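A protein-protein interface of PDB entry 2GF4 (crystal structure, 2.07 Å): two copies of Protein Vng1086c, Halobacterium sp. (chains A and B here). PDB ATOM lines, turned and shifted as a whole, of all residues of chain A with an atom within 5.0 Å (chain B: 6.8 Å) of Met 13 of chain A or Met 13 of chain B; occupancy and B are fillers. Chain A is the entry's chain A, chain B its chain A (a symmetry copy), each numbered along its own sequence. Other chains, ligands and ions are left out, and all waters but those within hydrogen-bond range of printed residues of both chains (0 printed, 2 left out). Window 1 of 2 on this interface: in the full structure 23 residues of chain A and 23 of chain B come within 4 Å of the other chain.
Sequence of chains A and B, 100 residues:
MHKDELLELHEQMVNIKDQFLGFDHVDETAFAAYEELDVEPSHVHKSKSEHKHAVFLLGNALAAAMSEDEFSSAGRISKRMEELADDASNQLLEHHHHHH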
ATOM      1  N   LEU A   9     -35.700  17.775   5.575  1.00  0.00           N
ATOM      2  CA  LEU A   9     -34.446  17.023   5.513  1.00  0.00           C
ATOM      3  C   LEU A   9     -34.678  15.681   6.201  1.00  0.00           C
ATOM      4  O   LEU A   9     -34.286  14.643   5.661  1.00  0.00           O
ATOM      5  CB  LEU A   9     -33.351  17.816   6.220  1.00  0.00           C
ATOM      6  CG  LEU A   9     -31.946  17.205   6.198  1.00  0.00           C
ATOM      7  CD1 LEU A   9     -31.478  17.084   4.797  1.00  0.00           C
ATOM      8  CD2 LEU A   9     -31.007  18.065   6.956  1.00  0.00           C
ATOM      9  N   HIS A  10     -35.276  15.691   7.388  1.00  0.00           N
ATOM     10  CA  HIS A  10     -35.573  14.457   8.095  1.00  0.00           C
ATOM     11  C   HIS A  10     -36.466  13.545   7.194  1.00  0.00           C
ATOM     12  O   HIS A  10     -36.153  12.359   7.066  1.00  0.00           O
ATOM     13  CB  HIS A  10     -36.254  14.818   9.403  1.00  0.00           C
ATOM     14  CG  HIS A  10     -36.399  13.677  10.361  1.00  0.00           C
ATOM     15  ND1 HIS A  10     -36.969  13.819  11.606  1.00  0.00           N
ATOM     16  CD2 HIS A  10     -36.079  12.368  10.242  1.00  0.00           C
ATOM     17  CE1 HIS A  10     -37.001  12.647  12.202  1.00  0.00           C
ATOM     18  NE2 HIS A  10     -36.465  11.753  11.401  1.00  0.00           N
ATOM     19  N   GLU A  11     -37.512  14.083   6.542  1.00  0.00           N
ATOM     20  CA  GLU A  11     -38.393  13.270   5.675  1.00  0.00           C
ATOM     21  C   GLU A  11     -37.583  12.576   4.603  1.00  0.00           C
ATOM     22  O   GLU A  11     -37.769  11.377   4.388  1.00  0.00           O
ATOM     23  CB  GLU A  11     -39.441  14.156   4.997  1.00  0.00           C
ATOM     24  CG  GLU A  11     -40.795  13.482   4.766  1.00  0.00           C
ATOM     25  CD  GLU A  11     -41.942  14.412   5.149  1.00  0.00           C
ATOM     26  OE1 GLU A  11     -42.836  14.013   5.931  1.00  0.00           O
ATOM     27  OE2 GLU A  11     -41.939  15.568   4.663  1.00  0.00           O
ATOM     28  N   GLN A  12     -36.695  13.309   3.928  1.00  0.00           N
ATOM     29  CA  GLN A  12     -35.902  12.696   2.874  1.00  0.00           C
ATOM     30  C   GLN A  12     -34.896  11.668   3.409  1.00  0.00           C
ATOM     31  O   GLN A  12     -34.693  10.639   2.756  1.00  0.00           O
ATOM     32  CB  GLN A  12     -35.199  13.780   2.054  1.00  0.00           C
ATOM     33  CG  GLN A  12     -36.154  14.584   1.160  1.00  0.00           C
ATOM     34  CD  GLN A  12     -37.011  13.719   0.246  1.00  0.00           C
ATOM     35  OE1 GLN A  12     -36.581  12.679  -0.245  1.00  0.00           O
ATOM     36  NE2 GLN A  12     -38.215  14.185  -0.011  1.00  0.00           N
ATOM     37  N   MET A  13     -34.276  11.912   4.563  1.00  0.00           N
ATOM     38  CA  MET A  13     -33.333  10.936   5.106  1.00  0.00           C
ATOM     39  C   MET A  13     -34.093   9.673   5.459  1.00  0.00           C
ATOM     40  O   MET A  13     -33.491   8.591   5.477  1.00  0.00           O
ATOM     41  CB  MET A  13     -32.649  11.494   6.340  1.00  0.00           C
ATOM     42  CG  MET A  13     -31.526  12.462   5.931  1.00  0.00           C
ATOM     43  SD  MET A  13     -30.090  11.541   4.805  1.00  0.00           S
ATOM     44  CE  MET A  13     -29.240  10.194   6.123  1.00  0.00           C
ATOM     45  N   VAL A  14     -35.385   9.779   5.764  1.00  0.00           N
ATOM     46  CA  VAL A  14     -36.134   8.570   6.066  1.00  0.00           C
ATOM     47  C   VAL A  14     -36.384   7.878   4.722  1.00  0.00           C
ATOM     48  O   VAL A  14     -36.396   6.633   4.672  1.00  0.00           O
ATOM     49  CB  VAL A  14     -37.386   8.918   6.820  1.00  0.00           C
ATOM     50  CG1 VAL A  14     -38.317   7.775   6.795  1.00  0.00           C
ATOM     51  CG2 VAL A  14     -36.986   9.195   8.250  1.00  0.00           C
ATOM     52  N   ASN A  15     -36.576   8.645   3.640  1.00  0.00           N
ATOM     53  CA  ASN A  15     -36.697   8.003   2.325  1.00  0.00           C
ATOM     54  C   ASN A  15     -35.369   7.265   2.050  1.00  0.00           C
ATOM     55  O   ASN A  15     -35.418   6.161   1.518  1.00  0.00           O
ATOM     56  CB  ASN A  15     -36.953   9.028   1.237  1.00  0.00           C
ATOM     57  CG  ASN A  15     -38.373   9.557   1.276  1.00  0.00           C
ATOM     58  OD1 ASN A  15     -38.711  10.503   0.593  1.00  0.00           O
ATOM     59  ND2 ASN A  15     -39.218   8.922   2.102  1.00  0.00           N
ATOM     60  N   ILE A  16     -34.196   7.827   2.391  1.00  0.00           N
ATOM     61  CA  ILE A  16     -32.920   7.131   2.155  1.00  0.00           C
ATOM     62  C   ILE A  16     -32.928   5.805   2.952  1.00  0.00           C
ATOM     63  O   ILE A  16     -32.636   4.741   2.393  1.00  0.00           O
ATOM     64  CB  ILE A  16     -31.742   8.026   2.613  1.00  0.00           C
ATOM     65  CG1 ILE A  16     -31.626   9.265   1.720  1.00  0.00           C
ATOM     66  CG2 ILE A  16     -30.483   7.260   2.554  1.00  0.00           C
ATOM     67  CD1 ILE A  16     -31.101   8.999   0.427  1.00  0.00           C
ATOM     68  N   LYS A  17     -33.253   5.869   4.247  1.00  0.00           N
ATOM     69  CA  LYS A  17     -33.315   4.686   5.092  1.00  0.00           C
ATOM     70  C   LYS A  17     -34.183   3.597   4.497  1.00  0.00           C
ATOM     71  O   LYS A  17     -33.770   2.441   4.483  1.00  0.00           O
ATOM     72  CB  LYS A  17     -33.903   5.049   6.430  1.00  0.00           C
ATOM     73  CG  LYS A  17     -34.146   3.812   7.209  1.00  0.00           C
ATOM     74  CD  LYS A  17     -34.057   4.083   8.636  1.00  0.00           C
ATOM     75  CE  LYS A  17     -35.356   4.554   9.102  1.00  0.00           C
ATOM     76  NZ  LYS A  17     -36.403   3.561   8.867  1.00  0.00           N
ATOM     77  N   VAL A  55     -31.677  13.545  12.402  1.00  0.00           N
ATOM     78  CA  VAL A  55     -30.959  13.523  11.132  1.00  0.00           C
ATOM     79  C   VAL A  55     -29.520  13.071  11.376  1.00  0.00           C
ATOM     80  O   VAL A  55     -28.958  12.347  10.552  1.00  0.00           O
ATOM     81  CB  VAL A  55     -31.044  14.880  10.477  1.00  0.00           C
ATOM     82  CG1 VAL A  55     -30.089  14.957   9.334  1.00  0.00           C
ATOM     83  CG2 VAL A  55     -32.454  15.052   9.954  1.00  0.00           C
ATOM     84  N   LEU A  58     -29.358   9.325  11.523  1.00  0.00           N
ATOM     85  CA  LEU A  58     -29.572   8.722  10.199  1.00  0.00           C
ATOM     86  C   LEU A  58     -28.317   8.830   9.347  1.00  0.00           C
ATOM     87  O   LEU A  58     -27.923   7.843   8.719  1.00  0.00           O
ATOM     88  CB  LEU A  58     -30.720   9.425   9.474  1.00  0.00           C
ATOM     89  CG  LEU A  58     -32.103   9.145  10.059  1.00  0.00           C
ATOM     90  CD1 LEU A  58     -33.134   9.906   9.321  1.00  0.00           C
ATOM     91  CD2 LEU A  58     -32.391   7.714   9.943  1.00  0.00           C
ATOM     92  N   GLY A  59     -27.721  10.025   9.291  1.00  0.00           N
ATOM     93  CA  GLY A  59     -26.495  10.205   8.516  1.00  0.00           C
ATOM     94  C   GLY A  59     -25.410   9.302   9.063  1.00  0.00           C
ATOM     95  O   GLY A  59     -24.744   8.588   8.325  1.00  0.00           O
ATOM     96  N   LEU A  62     -26.015   5.664   8.201  1.00  0.00           N
ATOM     97  CA  LEU A  62     -25.786   5.287   6.825  1.00  0.00           C
ATOM     98  C   LEU A  62     -24.275   5.139   6.652  1.00  0.00           C
ATOM     99  O   LEU A  62     -23.830   4.173   6.038  1.00  0.00           O
ATOM    100  CB  LEU A  62     -26.316   6.379   5.926  1.00  0.00           C
ATOM    101  CG  LEU A  62     -26.369   6.012   4.460  1.00  0.00           C
ATOM    102  CD1 LEU A  62     -27.409   4.940   4.247  1.00  0.00           C
ATOM    103  CD2 LEU A  62     -26.715   7.242   3.686  1.00  0.00           C
ATOM    104  N   GLU B   8     -27.786   4.184  -7.028  1.00  0.00           N
ATOM    105  CA  GLU B   8     -29.043   4.857  -6.712  1.00  0.00           C
ATOM    106  C   GLU B   8     -28.961   5.495  -5.330  1.00  0.00           C
ATOM    107  O   GLU B   8     -29.513   6.579  -5.130  1.00  0.00           O
ATOM    108  CB  GLU B   8     -30.198   3.854  -6.810  1.00  0.00           C
ATOM    109  CG  GLU B   8     -30.528   3.525  -8.278  1.00  0.00           C
ATOM    110  CD  GLU B   8     -31.553   2.411  -8.450  1.00  0.00           C
ATOM    111  OE1 GLU B   8     -32.768   2.689  -8.412  1.00  0.00           O
ATOM    112  OE2 GLU B   8     -31.145   1.243  -8.630  1.00  0.00           O
ATOM    113  N   LEU B   9     -28.274   4.851  -4.390  1.00  0.00           N
ATOM    114  CA  LEU B   9     -28.140   5.412  -3.045  1.00  0.00           C
ATOM    115  C   LEU B   9     -27.279   6.666  -3.152  1.00  0.00           C
ATOM    116  O   LEU B   9     -27.632   7.699  -2.576  1.00  0.00           O
ATOM    117  CB  LEU B   9     -27.484   4.377  -2.134  1.00  0.00           C
ATOM    118  CG  LEU B   9     -27.321   4.771  -0.663  1.00  0.00           C
ATOM    119  CD1 LEU B   9     -28.654   5.012  -0.062  1.00  0.00           C
ATOM    120  CD2 LEU B   9     -26.636   3.687   0.079  1.00  0.00           C
ATOM    121  N   HIS B  10     -26.149   6.583  -3.847  1.00  0.00           N
ATOM    122  CA  HIS B  10     -25.290   7.739  -4.035  1.00  0.00           C
ATOM    123  C   HIS B  10     -26.105   8.887  -4.712  1.00  0.00           C
ATOM    124  O   HIS B  10     -26.035  10.021  -4.231  1.00  0.00           O
ATOM    125  CB  HIS B  10     -24.098   7.308  -4.872  1.00  0.00           C
ATOM    126  CG  HIS B  10     -22.995   8.317  -4.943  1.00  0.00           C
ATOM    127  ND1 HIS B  10     -21.825   8.092  -5.635  1.00  0.00           N
ATOM    128  CD2 HIS B  10     -22.897   9.568  -4.439  1.00  0.00           C
ATOM    129  CE1 HIS B  10     -21.067   9.164  -5.560  1.00  0.00           C
ATOM    130  NE2 HIS B  10     -21.690  10.070  -4.838  1.00  0.00           N
ATOM    131  N   GLU B  11     -26.898   8.604  -5.761  1.00  0.00           N
ATOM    132  CA  GLU B  11     -27.694   9.648  -6.443  1.00  0.00           C
ATOM    133  C   GLU B  11     -28.595  10.354  -5.454  1.00  0.00           C
ATOM    134  O   GLU B  11     -28.643  11.585  -5.456  1.00  0.00           O
ATOM    135  CB  GLU B  11     -28.564   9.026  -7.538  1.00  0.00           C
ATOM    136  CG  GLU B  11     -28.784   9.918  -8.762  1.00  0.00           C
ATOM    137  CD  GLU B  11     -28.621   9.123 -10.054  1.00  0.00           C
ATOM    138  OE1 GLU B  11     -27.851   9.540 -10.951  1.00  0.00           O
ATOM    139  OE2 GLU B  11     -29.271   8.057 -10.166  1.00  0.00           O
ATOM    140  N   GLN B  12     -29.309   9.597  -4.618  1.00  0.00           N
ATOM    141  CA  GLN B  12     -30.205  10.225  -3.660  1.00  0.00           C
ATOM    142  C   GLN B  12     -29.457  11.010  -2.575  1.00  0.00           C
ATOM    143  O   GLN B  12     -29.936  12.077  -2.176  1.00  0.00           O
ATOM    144  CB  GLN B  12     -31.126   9.171  -3.042  1.00  0.00           C
ATOM    145  CG  GLN B  12     -32.192   8.645  -4.015  1.00  0.00           C
ATOM    146  CD  GLN B  12     -33.023   9.744  -4.662  1.00  0.00           C
ATOM    147  OE1 GLN B  12     -33.325  10.766  -4.053  1.00  0.00           O
ATOM    148  NE2 GLN B  12     -33.428   9.499  -5.891  1.00  0.00           N
ATOM    149  N   MET B  13     -28.313  10.522  -2.097  1.00  0.00           N
ATOM    150  CA  MET B  13     -27.569  11.266  -1.082  1.00  0.00           C
ATOM    151  C   MET B  13     -27.085  12.567  -1.691  1.00  0.00           C
ATOM    152  O   MET B  13     -26.867  13.536  -0.951  1.00  0.00           O
ATOM    153  CB  MET B  13     -26.387  10.450  -0.591  1.00  0.00           C
ATOM    154  CG  MET B  13     -26.857   9.392   0.421  1.00  0.00           C
ATOM    155  SD  MET B  13     -27.736  10.236   2.062  1.00  0.00           S
ATOM    156  CE  MET B  13     -26.179  11.251   2.968  1.00  0.00           C
ATOM    157  N   VAL B  14     -26.888  12.612  -3.007  1.00  0.00           N
ATOM    158  CA  VAL B  14     -26.463  13.866  -3.609  1.00  0.00           C
ATOM    159  C   VAL B  14     -27.704  14.764  -3.642  1.00  0.00           C
ATOM    160  O   VAL B  14     -27.570  15.991  -3.480  1.00  0.00           O
ATOM    161  CB  VAL B  14     -25.854  13.606  -4.957  1.00  0.00           C
ATOM    162  CG1 VAL B  14     -25.774  14.867  -5.718  1.00  0.00           C
ATOM    163  CG2 VAL B  14     -24.458  13.081  -4.727  1.00  0.00           C
ATOM    164  N   ASN B  15     -28.897  14.187  -3.841  1.00  0.00           N
ATOM    165  CA  ASN B  15     -30.109  15.014  -3.757  1.00  0.00           C
ATOM    166  C   ASN B  15     -30.182  15.578  -2.322  1.00  0.00           C
ATOM    167  O   ASN B  15     -30.546  16.739  -2.173  1.00  0.00           O
ATOM    168  CB  ASN B  15     -31.350  14.195  -4.054  1.00  0.00           C
ATOM    169  CG  ASN B  15     -31.486  13.881  -5.530  1.00  0.00           C
ATOM    170  OD1 ASN B  15     -32.323  13.097  -5.932  1.00  0.00           O
ATOM    171  ND2 ASN B  15     -30.635  14.515  -6.350  1.00  0.00           N
ATOM    172  N   ILE B  16     -29.848  14.808  -1.271  1.00  0.00           N
ATOM    173  CA  ILE B  16     -29.892  15.335   0.104  1.00  0.00           C
ATOM    174  C   ILE B  16     -28.910  16.526   0.206  1.00  0.00           C
ATOM    175  O   ILE B  16     -29.286  17.602   0.689  1.00  0.00           O
ATOM    176  CB  ILE B  16     -29.492  14.222   1.104  1.00  0.00           C
ATOM    177  CG1 ILE B  16     -30.549  13.113   1.128  1.00  0.00           C
ATOM    178  CG2 ILE B  16     -29.352  14.794   2.456  1.00  0.00           C
ATOM    179  CD1 ILE B  16     -31.749  13.472   1.796  1.00  0.00           C
ATOM    180  N   LYS B  17     -27.664  16.335  -0.237  1.00  0.00           N
ATOM    181  CA  LYS B  17     -26.660  17.388  -0.212  1.00  0.00           C
ATOM    182  C   LYS B  17     -27.146  18.664  -0.868  1.00  0.00           C
ATOM    183  O   LYS B  17     -26.961  19.737  -0.301  1.00  0.00           O
ATOM    184  CB  LYS B  17     -25.434  16.937  -0.960  1.00  0.00           C
ATOM    185  CG  LYS B  17     -24.498  18.079  -1.099  1.00  0.00           C
ATOM    186  CD  LYS B  17     -23.125  17.606  -1.174  1.00  0.00           C
ATOM    187  CE  LYS B  17     -22.822  17.271  -2.561  1.00  0.00           C
ATOM    188  NZ  LYS B  17     -22.979  18.431  -3.439  1.00  0.00           N
ATOM    189  N   ASP B  18     -27.740  18.558  -2.059  1.00  0.00           N
ATOM    190  CA  ASP B  18     -28.205  19.760  -2.732  1.00  0.00           C
ATOM    191  C   ASP B  18     -29.322  20.401  -1.950  1.00  0.00           C
ATOM    192  O   ASP B  18     -29.348  21.626  -1.839  1.00  0.00           O
ATOM    193  CB  ASP B  18     -28.564  19.418  -4.162  1.00  0.00           C
ATOM    194  CG  ASP B  18     -27.314  19.131  -4.989  1.00  0.00           C
ATOM    195  OD1 ASP B  18     -26.220  19.638  -4.653  1.00  0.00           O
ATOM    196  OD2 ASP B  18     -27.385  18.411  -5.988  1.00  0.00           O
ATOM    197  N   GLN B  19     -30.224  19.584  -1.399  1.00  0.00           N
ATOM    198  CA  GLN B  19     -31.327  20.040  -0.552  1.00  0.00           C
ATOM    199  C   GLN B  19     -30.724  20.861   0.609  1.00  0.00           C
ATOM    200  O   GLN B  19     -31.126  22.005   0.815  1.00  0.00           O
ATOM    201  CB  GLN B  19     -32.031  18.816   0.020  1.00  0.00           C
ATOM    202  CG  GLN B  19     -33.289  19.183   0.726  1.00  0.00           C
ATOM    203  CD  GLN B  19     -33.996  18.013   1.360  1.00  0.00           C
ATOM    204  OE1 GLN B  19     -33.520  16.875   1.348  1.00  0.00           O
ATOM    205  NE2 GLN B  19     -35.141  18.305   1.931  1.00  0.00           N
ATOM    206  N   PHE B  31     -19.527  19.633   2.859  1.00  0.00           N
ATOM    207  CA  PHE B  31     -19.182  18.422   2.156  1.00  0.00           C
ATOM    208  C   PHE B  31     -17.842  18.494   1.495  1.00  0.00           C
ATOM    209  O   PHE B  31     -17.622  17.807   0.495  1.00  0.00           O
ATOM    210  CB  PHE B  31     -20.278  18.114   1.152  1.00  0.00           C
ATOM    211  CG  PHE B  31     -21.607  17.927   1.793  1.00  0.00           C
ATOM    212  CD1 PHE B  31     -22.478  18.984   1.945  1.00  0.00           C
ATOM    213  CD2 PHE B  31     -21.984  16.686   2.262  1.00  0.00           C
ATOM    214  CE1 PHE B  31     -23.684  18.801   2.548  1.00  0.00           C
ATOM    215  CE2 PHE B  31     -23.192  16.517   2.864  1.00  0.00           C
ATOM    216  CZ  PHE B  31     -24.038  17.570   3.003  1.00  0.00           C
ATOM    217  N   ALA B  54     -17.941   7.231  -1.235  1.00  0.00           N
ATOM    218  CA  ALA B  54     -18.644   8.496  -1.435  1.00  0.00           C
ATOM    219  C   ALA B  54     -19.906   8.560  -0.591  1.00  0.00           C
ATOM    220  O   ALA B  54     -20.212   9.619  -0.052  1.00  0.00           O
ATOM    221  CB  ALA B  54     -19.003   8.684  -2.918  1.00  0.00           C
ATOM    222  N   VAL B  55     -20.642   7.472  -0.445  1.00  0.00           N
ATOM    223  CA  VAL B  55     -21.843   7.561   0.378  1.00  0.00           C
ATOM    224  C   VAL B  55     -21.438   7.758   1.838  1.00  0.00           C
ATOM    225  O   VAL B  55     -22.106   8.497   2.563  1.00  0.00           O
ATOM    226  CB  VAL B  55     -22.695   6.333   0.167  1.00  0.00           C
ATOM    227  CG1 VAL B  55     -23.769   6.273   1.199  1.00  0.00           C
ATOM    228  CG2 VAL B  55     -23.332   6.443  -1.202  1.00  0.00           C
ATOM    229  N   PHE B  56     -20.356   7.110   2.257  1.00  0.00           N
ATOM    230  CA  PHE B  56     -19.831   7.277   3.615  1.00  0.00           C
ATOM    231  C   PHE B  56     -19.540   8.761   3.868  1.00  0.00           C
ATOM    232  O   PHE B  56     -19.988   9.322   4.869  1.00  0.00           O
ATOM    233  CB  PHE B  56     -18.525   6.496   3.727  1.00  0.00           C
ATOM    234  CG  PHE B  56     -17.867   6.640   5.048  1.00  0.00           C
ATOM    235  CD1 PHE B  56     -16.934   7.636   5.278  1.00  0.00           C
ATOM    236  CD2 PHE B  56     -18.137   5.739   6.059  1.00  0.00           C
ATOM    237  CE1 PHE B  56     -16.334   7.749   6.504  1.00  0.00           C
ATOM    238  CE2 PHE B  56     -17.536   5.857   7.279  1.00  0.00           C
ATOM    239  CZ  PHE B  56     -16.627   6.846   7.498  1.00  0.00           C
ATOM    240  N   LEU B  57     -18.790   9.405   2.976  1.00  0.00           N
ATOM    241  CA  LEU B  57     -18.467  10.807   3.182  1.00  0.00           C
ATOM    242  C   LEU B  57     -19.680  11.715   3.255  1.00  0.00           C
ATOM    243  O   LEU B  57     -19.654  12.714   3.987  1.00  0.00           O
ATOM    244  CB  LEU B  57     -17.529  11.266   2.081  1.00  0.00           C
ATOM    245  CG  LEU B  57     -16.129  10.665   2.269  1.00  0.00           C
ATOM    246  CD1 LEU B  57     -15.338  10.985   1.046  1.00  0.00           C
ATOM    247  CD2 LEU B  57     -15.449  11.221   3.519  1.00  0.00           C
ATOM    248  N   LEU B  58     -20.730  11.384   2.494  1.00  0.00           N
ATOM    249  CA  LEU B  58     -21.963  12.187   2.482  1.00  0.00           C
ATOM    250  C   LEU B  58     -22.734  12.013   3.781  1.00  0.00           C
ATOM    251  O   LEU B  58     -23.181  13.007   4.360  1.00  0.00           O
ATOM    252  CB  LEU B  58     -22.859  11.766   1.317  1.00  0.00           C
ATOM    253  CG  LEU B  58     -22.335  12.165  -0.060  1.00  0.00           C
ATOM    254  CD1 LEU B  58     -23.244  11.672  -1.116  1.00  0.00           C
ATOM    255  CD2 LEU B  58     -22.258  13.625  -0.140  1.00  0.00           C
ATOM    256  N   GLY B  59     -22.925  10.761   4.211  1.00  0.00           N
ATOM    257  CA  GLY B  59     -23.633  10.510   5.465  1.00  0.00           C
ATOM    258  C   GLY B  59     -22.886  11.160   6.610  1.00  0.00           C
ATOM    259  O   GLY B  59     -23.465  11.862   7.429  1.00  0.00           O
ATOM    260  N   ASN B  60     -21.597  10.902   6.680  1.00  0.00           N
ATOM    261  CA  ASN B  60     -20.778  11.474   7.698  1.00  0.00           C
ATOM    262  C   ASN B  60     -20.870  12.966   7.725  1.00  0.00           C
ATOM    263  O   ASN B  60     -20.969  13.575   8.786  1.00  0.00           O
ATOM    264  CB  ASN B  60     -19.391  11.122   7.392  1.00  0.00           C
ATOM    265  CG  ASN B  60     -18.692  10.720   8.562  1.00  0.00           C
ATOM    266  OD1 ASN B  60     -17.868  11.448   9.082  1.00  0.00           O
ATOM    267  ND2 ASN B  60     -19.036   9.550   9.055  1.00  0.00           N
ATOM    268  N   LEU B  62     -23.242  14.930   6.585  1.00  0.00           N
ATOM    269  CA  LEU B  62     -24.529  15.454   6.983  1.00  0.00           C
ATOM    270  C   LEU B  62     -24.576  15.399   8.510  1.00  0.00           C
ATOM    271  O   LEU B  62     -25.009  16.364   9.134  1.00  0.00           O
ATOM    272  CB  LEU B  62     -25.613  14.584   6.391  1.00  0.00           C
ATOM    273  CG  LEU B  62     -27.009  15.151   6.517  1.00  0.00           C
ATOM    274  CD1 LEU B  62     -27.132  16.383   5.656  1.00  0.00           C
ATOM    275  CD2 LEU B  62     -27.978  14.103   6.077  1.00  0.00           C
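Gln 12 of chain A touches Ile 16 of chain B, and with the chains exchanged Ile 16 of chain A touches Gln 12 of chain B. Met 13 of chain A touches its own counterpart, Met 13 of chain B. Met 13 of chain A touches Ile 16 of chain B, and with the chains exchanged Ile 16 of chain A touches Met 13 of chain B. Val 55 of chain A touches Leu 62 of chain B, and with the chains exchanged Leu 62 of chain A touches Val 55 of chain B. 13 positions are printed for both chains. Of the 14 pairs that touch across the chains among the printed residues, 12 have their exchanged pair printed and touching as well.
Of chain B, only Met 13 (3.8 Å), Ile 16 (3.9 Å) and Leu 62 (3.6 Å) come within 4 Å of Met 13 of chain A. Of chain A, only Met 13, Ile 16 and Leu 62 come within 4 Å of Met 13 of chain B. Of the printed residues of chain B, Ile 16 of chain A touches Leu 9, Gln 12 and Met 13. Printed residues of chain B within 4 Å of Gly 59 of chain A: Gly 59. Of the printed residues of chain B, Leu 9 of chain A touches Ile 16 and Gln 19. Printed residues of chain A within 4 Å of Gln 19 of chain B: Leu 9 and Gln 12. The nearest residue of chain B that does not touch Met 13 of chain A is Gly 59 of chain B (5.7 Å). The nearest printed residue of chain A that does not touch Met 13 of chain B is Gly 59 of chain A (5.7 Å). The nearest printed residue of chain A that does not touch Ile 16 of chain B is Ile 16 of chain A (4.04 Å).
CD1 of Leu 9 of chain A touches CG2 of Ile 16 of chain B, 3.9 Å away. Ile 16 of chain B touches Gln 12 of chain A. Gln 12 of chain A touches Gln 19 of chain B. Ile 16 of chain B touches Met 13 of chain A (CD1 to SD, 3.9 Å). Leu 62 of chain B touches Met 13 of chain A. CB of Gln 12 of chain B touches CD1 of Ile 16 of chain A, at 3.5 Å. Ile 16 of chain A touches Met 13 of chain B. Gly 59 of chain B touches Gly 59 of chain A (O to C, 3.6 Å). Leu 62 of chain A touches Met 13 of chain B. Leu 62 of chain A touches Val 55 of chain B (CD2 to CG1, 3.98 Å).
Hydrophobic or aromatic side chains of chain A within 4 Å of the printed part of chain B: Leu 9, Met 13, Ile 16, Val 55 and Leu 62. Printed residues of chain B that touch a printed residue of chain A: Leu 9, Gln 12, Met 13, Ile 16, Gln 19, Val 55, Gly 59 and Leu 62. Among the printed residues, 14 pairs touch across the chains.
OE1 of Gln 12 of chain A lies close to OD1 of Asn 15 of chain A (3.2 Å). The side-chain amide oxygen of Gln 12 of chain B sits close to the side-chain amide oxygen of Asn 15 of chain B.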
